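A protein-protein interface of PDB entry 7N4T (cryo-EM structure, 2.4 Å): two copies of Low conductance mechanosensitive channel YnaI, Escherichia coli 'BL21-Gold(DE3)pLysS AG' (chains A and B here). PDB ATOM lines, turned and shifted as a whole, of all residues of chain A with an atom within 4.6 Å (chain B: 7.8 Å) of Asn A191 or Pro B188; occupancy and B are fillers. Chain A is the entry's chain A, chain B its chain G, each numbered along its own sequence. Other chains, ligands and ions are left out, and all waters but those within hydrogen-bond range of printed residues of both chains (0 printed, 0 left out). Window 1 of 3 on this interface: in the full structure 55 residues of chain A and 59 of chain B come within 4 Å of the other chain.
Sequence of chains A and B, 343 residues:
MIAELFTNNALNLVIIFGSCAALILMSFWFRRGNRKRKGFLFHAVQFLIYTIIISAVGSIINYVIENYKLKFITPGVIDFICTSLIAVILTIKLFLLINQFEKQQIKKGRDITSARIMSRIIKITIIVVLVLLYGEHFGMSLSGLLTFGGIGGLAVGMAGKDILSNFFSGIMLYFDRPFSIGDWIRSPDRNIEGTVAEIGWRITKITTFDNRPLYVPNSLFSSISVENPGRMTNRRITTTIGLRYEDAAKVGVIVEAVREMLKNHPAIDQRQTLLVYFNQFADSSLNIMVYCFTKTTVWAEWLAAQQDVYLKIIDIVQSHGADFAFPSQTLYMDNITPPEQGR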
ATOM      1  N   ARG A 190      -3.567  -0.646   5.068  1.00  0.00           N
ATOM      2  CA  ARG A 190      -4.522  -0.231   4.052  1.00  0.00           C
ATOM      3  C   ARG A 190      -5.140   1.104   4.436  1.00  0.00           C
ATOM      4  O   ARG A 190      -5.097   1.517   5.598  1.00  0.00           O
ATOM      5  CB  ARG A 190      -5.620  -1.283   3.865  1.00  0.00           C
ATOM      6  CG  ARG A 190      -5.257  -2.355   2.858  1.00  0.00           C
ATOM      7  CD  ARG A 190      -6.319  -3.431   2.773  1.00  0.00           C
ATOM      8  NE  ARG A 190      -7.402  -3.056   1.872  1.00  0.00           N
ATOM      9  CZ  ARG A 190      -8.001  -3.878   1.022  1.00  0.00           C
ATOM     10  NH1 ARG A 190      -7.643  -5.148   0.911  1.00  0.00           N
ATOM     11  NH2 ARG A 190      -8.985  -3.416   0.257  1.00  0.00           N
ATOM     12  N   ASN A 191      -5.717   1.775   3.442  1.00  0.00           N
ATOM     13  CA  ASN A 191      -6.327   3.089   3.632  1.00  0.00           C
ATOM     14  C   ASN A 191      -7.787   2.904   4.022  1.00  0.00           C
ATOM     15  O   ASN A 191      -8.652   2.707   3.167  1.00  0.00           O
ATOM     16  CB  ASN A 191      -6.198   3.923   2.364  1.00  0.00           C
ATOM     17  CG  ASN A 191      -6.610   5.365   2.571  1.00  0.00           C
ATOM     18  OD1 ASN A 191      -7.315   5.693   3.525  1.00  0.00           O
ATOM     19  ND2 ASN A 191      -6.174   6.239   1.672  1.00  0.00           N
ATOM     20  N   ILE A 192      -8.064   2.968   5.322  1.00  0.00           N
ATOM     21  CA  ILE A 192      -9.429   2.900   5.832  1.00  0.00           C
ATOM     22  C   ILE A 192      -9.656   4.057   6.795  1.00  0.00           C
ATOM     23  O   ILE A 192     -10.553   4.004   7.643  1.00  0.00           O
ATOM     24  CB  ILE A 192      -9.703   1.548   6.517  1.00  0.00           C
ATOM     25  CG1 ILE A 192      -8.725   1.323   7.673  1.00  0.00           C
ATOM     26  CG2 ILE A 192      -9.601   0.418   5.509  1.00  0.00           C
ATOM     27  CD1 ILE A 192      -9.054   0.120   8.521  1.00  0.00           C
ATOM     28  N   GLU A 193      -8.848   5.106   6.673  1.00  0.00           N
ATOM     29  CA  GLU A 193      -8.868   6.180   7.654  1.00  0.00           C
ATOM     30  C   GLU A 193     -10.198   6.921   7.627  1.00  0.00           C
ATOM     31  O   GLU A 193     -10.786   7.143   6.565  1.00  0.00           O
ATOM     32  CB  GLU A 193      -7.723   7.156   7.392  1.00  0.00           C
ATOM     33  CG  GLU A 193      -7.422   8.073   8.566  1.00  0.00           C
ATOM     34  CD  GLU A 193      -5.974   8.518   8.613  1.00  0.00           C
ATOM     35  OE1 GLU A 193      -5.173   8.051   7.777  1.00  0.00           O
ATOM     36  OE2 GLU A 193      -5.634   9.338   9.491  1.00  0.00           O
ATOM     37  N   LEU A 214     -17.339   5.759   3.191  1.00  0.00           N
ATOM     38  CA  LEU A 214     -16.402   4.721   2.784  1.00  0.00           C
ATOM     39  C   LEU A 214     -16.923   3.399   3.319  1.00  0.00           C
ATOM     40  O   LEU A 214     -17.136   3.260   4.525  1.00  0.00           O
ATOM     41  CB  LEU A 214     -14.996   5.008   3.318  1.00  0.00           C
ATOM     42  CG  LEU A 214     -13.897   4.004   2.967  1.00  0.00           C
ATOM     43  CD1 LEU A 214     -13.550   4.066   1.493  1.00  0.00           C
ATOM     44  CD2 LEU A 214     -12.665   4.255   3.816  1.00  0.00           C
ATOM     45  N   ARG B 186     -15.108   5.886  -6.077  1.00  0.00           N
ATOM     46  CA  ARG B 186     -13.674   5.693  -6.216  1.00  0.00           C
ATOM     47  C   ARG B 186     -13.222   4.743  -5.120  1.00  0.00           C
ATOM     48  O   ARG B 186     -13.947   4.495  -4.155  1.00  0.00           O
ATOM     49  CB  ARG B 186     -12.915   7.021  -6.145  1.00  0.00           C
ATOM     50  CG  ARG B 186     -12.974   7.705  -4.790  1.00  0.00           C
ATOM     51  CD  ARG B 186     -12.178   8.997  -4.791  1.00  0.00           C
ATOM     52  NE  ARG B 186     -10.762   8.763  -5.045  1.00  0.00           N
ATOM     53  CZ  ARG B 186      -9.924   8.217  -4.175  1.00  0.00           C
ATOM     54  NH1 ARG B 186     -10.323   7.848  -2.969  1.00  0.00           N
ATOM     55  NH2 ARG B 186      -8.653   8.037  -4.524  1.00  0.00           N
ATOM     56  N   SER B 187     -12.015   4.208  -5.282  1.00  0.00           N
ATOM     57  CA  SER B 187     -11.477   3.264  -4.319  1.00  0.00           C
ATOM     58  C   SER B 187     -10.007   3.560  -4.056  1.00  0.00           C
ATOM     59  O   SER B 187      -9.232   3.737  -5.003  1.00  0.00           O
ATOM     60  CB  SER B 187     -11.627   1.823  -4.824  1.00  0.00           C
ATOM     61  OG  SER B 187     -11.186   0.897  -3.849  1.00  0.00           O
ATOM     62  N   PRO B 188      -9.591   3.630  -2.788  1.00  0.00           N
ATOM     63  CA  PRO B 188      -8.150   3.769  -2.520  1.00  0.00           C
ATOM     64  C   PRO B 188      -7.336   2.601  -3.045  1.00  0.00           C
ATOM     65  O   PRO B 188      -6.163   2.777  -3.396  1.00  0.00           O
ATOM     66  CB  PRO B 188      -8.076   3.871  -0.989  1.00  0.00           C
ATOM     67  CG  PRO B 188      -9.459   4.142  -0.524  1.00  0.00           C
ATOM     68  CD  PRO B 188     -10.389   3.605  -1.551  1.00  0.00           C
ATOM     69  N   ASP B 189      -7.927   1.406  -3.105  1.00  0.00           N
ATOM     70  CA  ASP B 189      -7.164   0.219  -3.474  1.00  0.00           C
ATOM     71  C   ASP B 189      -7.001   0.101  -4.985  1.00  0.00           C
ATOM     72  O   ASP B 189      -5.914  -0.226  -5.473  1.00  0.00           O
ATOM     73  CB  ASP B 189      -7.845  -1.028  -2.915  1.00  0.00           C
ATOM     74  CG  ASP B 189      -8.066  -0.948  -1.419  1.00  0.00           C
ATOM     75  OD1 ASP B 189      -9.208  -1.184  -0.972  1.00  0.00           O
ATOM     76  OD2 ASP B 189      -7.099  -0.650  -0.687  1.00  0.00           O
ATOM     77  N   ARG B 190      -8.064   0.361  -5.739  1.00  0.00           N
ATOM     78  CA  ARG B 190      -8.079   0.165  -7.180  1.00  0.00           C
ATOM     79  C   ARG B 190      -8.520   1.443  -7.884  1.00  0.00           C
ATOM     80  O   ARG B 190      -8.982   2.400  -7.260  1.00  0.00           O
ATOM     81  CB  ARG B 190      -9.009  -0.995  -7.553  1.00  0.00           C
ATOM     82  CG  ARG B 190      -8.328  -2.349  -7.573  1.00  0.00           C
ATOM     83  CD  ARG B 190      -9.276  -3.437  -8.044  1.00  0.00           C
ATOM     84  NE  ARG B 190      -8.566  -4.563  -8.642  1.00  0.00           N
ATOM     85  CZ  ARG B 190      -8.450  -4.781  -9.946  1.00  0.00           C
ATOM     86  NH1 ARG B 190      -8.977  -3.959 -10.838  1.00  0.00           N
ATOM     87  NH2 ARG B 190      -7.784  -5.852 -10.365  1.00  0.00           N
ATOM     88  N   ASN B 191      -8.369   1.443  -9.203  1.00  0.00           N
ATOM     89  CA  ASN B 191      -8.740   2.573 -10.051  1.00  0.00           C
ATOM     90  C   ASN B 191     -10.084   2.249 -10.700  1.00  0.00           C
ATOM     91  O   ASN B 191     -10.147   1.612 -11.752  1.00  0.00           O
ATOM     92  CB  ASN B 191      -7.665   2.846 -11.098  1.00  0.00           C
ATOM     93  CG  ASN B 191      -7.905   4.134 -11.857  1.00  0.00           C
ATOM     94  OD1 ASN B 191      -9.043   4.574 -12.017  1.00  0.00           O
ATOM     95  ND2 ASN B 191      -6.830   4.749 -12.333  1.00  0.00           N
ATOM     96  N   ILE B 192     -11.163   2.694 -10.058  1.00  0.00           N
ATOM     97  CA  ILE B 192     -12.512   2.510 -10.576  1.00  0.00           C
ATOM     98  C   ILE B 192     -13.236   3.849 -10.570  1.00  0.00           C
ATOM     99  O   ILE B 192     -14.470   3.899 -10.565  1.00  0.00           O
ATOM    100  CB  ILE B 192     -13.285   1.460  -9.758  1.00  0.00           C
ATOM    101  CG1 ILE B 192     -13.394   1.893  -8.292  1.00  0.00           C
ATOM    102  CG2 ILE B 192     -12.604   0.107  -9.858  1.00  0.00           C
ATOM    103  CD1 ILE B 192     -14.332   1.040  -7.477  1.00  0.00           C
ATOM    104  N   ILE B 224     -12.491  -4.619  -1.846  1.00  0.00           N
ATOM    105  CA  ILE B 224     -11.902  -3.289  -1.813  1.00  0.00           C
ATOM    106  C   ILE B 224     -12.850  -2.355  -1.076  1.00  0.00           C
ATOM    107  O   ILE B 224     -14.057  -2.588  -0.997  1.00  0.00           O
ATOM    108  CB  ILE B 224     -11.602  -2.741  -3.225  1.00  0.00           C
ATOM    109  CG1 ILE B 224     -12.905  -2.453  -3.976  1.00  0.00           C
ATOM    110  CG2 ILE B 224     -10.741  -3.725  -3.998  1.00  0.00           C
ATOM    111  CD1 ILE B 224     -12.710  -2.095  -5.431  1.00  0.00           C
ATOM    112  N   SER B 225     -12.280  -1.284  -0.533  1.00  0.00           N
ATOM    113  CA  SER B 225     -13.069  -0.248   0.118  1.00  0.00           C
ATOM    114  C   SER B 225     -13.585   0.716  -0.942  1.00  0.00           C
ATOM    115  O   SER B 225     -12.795   1.364  -1.635  1.00  0.00           O
ATOM    116  CB  SER B 225     -12.230   0.490   1.156  1.00  0.00           C
ATOM    117  OG  SER B 225     -11.599  -0.420   2.038  1.00  0.00           O
ATOM    118  N   VAL B 226     -14.903   0.807  -1.071  1.00  0.00           N
ATOM    119  CA  VAL B 226     -15.538   1.665  -2.061  1.00  0.00           C
ATOM    120  C   VAL B 226     -15.905   2.976  -1.383  1.00  0.00           C
ATOM    121  O   VAL B 226     -16.673   2.990  -0.414  1.00  0.00           O
ATOM    122  CB  VAL B 226     -16.778   0.996  -2.674  1.00  0.00           C
ATOM    123  CG1 VAL B 226     -17.548   1.991  -3.529  1.00  0.00           C
ATOM    124  CG2 VAL B 226     -16.371  -0.223  -3.489  1.00  0.00           C
ATOM    125  N   GLU B 227     -15.357   4.072  -1.889  1.00  0.00           N
ATOM    126  CA  GLU B 227     -15.671   5.403  -1.399  1.00  0.00           C
ATOM    127  C   GLU B 227     -16.650   6.064  -2.359  1.00  0.00           C
ATOM    128  O   GLU B 227     -16.560   5.898  -3.577  1.00  0.00           O
ATOM    129  CB  GLU B 227     -14.399   6.242  -1.262  1.00  0.00           C
ATOM    130  CG  GLU B 227     -14.630   7.703  -0.927  1.00  0.00           C
ATOM    131  CD  GLU B 227     -13.334   8.469  -0.771  1.00  0.00           C
ATOM    132  OE1 GLU B 227     -12.364   7.896  -0.232  1.00  0.00           O
ATOM    133  OE2 GLU B 227     -13.279   9.644  -1.189  1.00  0.00           O
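Positions printed for both chains: 190, 191 and 192.
Of the 6 pairs that touch across the chains among the printed residues, none has its exchanged pair printed and touching as well.
Hydrophobic or aromatic side chains of chain A that line the printed part of chain B: Leu A214.
Printed residues of chain B that touch a printed residue of chain A: Pro B188, Asp B189, Ile B224, Ser B225, Val B226 and Glu B227.
Hydrophobic or aromatic side chains of chain B that line the printed part of chain A: Pro B188.
Among the printed residues, 6 pairs touch across the chains.
Among the printed residues, Asp or Glu carboxylates within 4 Å of a Lys or Arg side-chain nitrogen of the other chain: Arg A190 with Asp B189 (2.6 Å).
The side-chain hydroxyl of Ser B187 is in hydrogen-bond range of the backbone carbonyl oxygen of Ser B225.
The guanidinium group (NH1) of Arg B186 lies within salt-bridge range of the side-chain carboxylate (OE1) of Glu B227.
OG of Ser B187 lies close to N of Asp B189, at 3.4 Å.
The side-chain carboxylate (OD1) of Asp B189 sits at hydrogen-bond distance from the backbone NH (N) of Ser B225 (3.1 Å).
Of the printed residues of chain B, Arg A190 touches Asp B189 and Ile B224.
Asn A191 touches just one residue of chain B: Pro B188 (3.8 Å).
Of the printed residues of chain A, Asp B189 touches Arg A190 (2.6 Å).
Of the printed residues of chain A, Ile B224 touches Arg A190.
Of the printed residues of chain A, Val B226 touches Leu A214 (3.6 Å).
Of the printed residues of chain A, Glu B227 touches Leu A214 (3.6 Å).
The nearest residue of chain A that does not touch Pro B188 is Leu A214 (4.4 Å).
Among the printed residues, pairs that only touch across the chains: Arg A190 with Ile B224, Leu A214 with Glu B227, Leu A214 with Val B226, Leu A214 with Ser B225 and Asn A191 with Pro B188.
The guanidinium group of Arg A190 lies within salt-bridge range of the side-chain carboxylate of Asp B189, at 2.6 Å.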
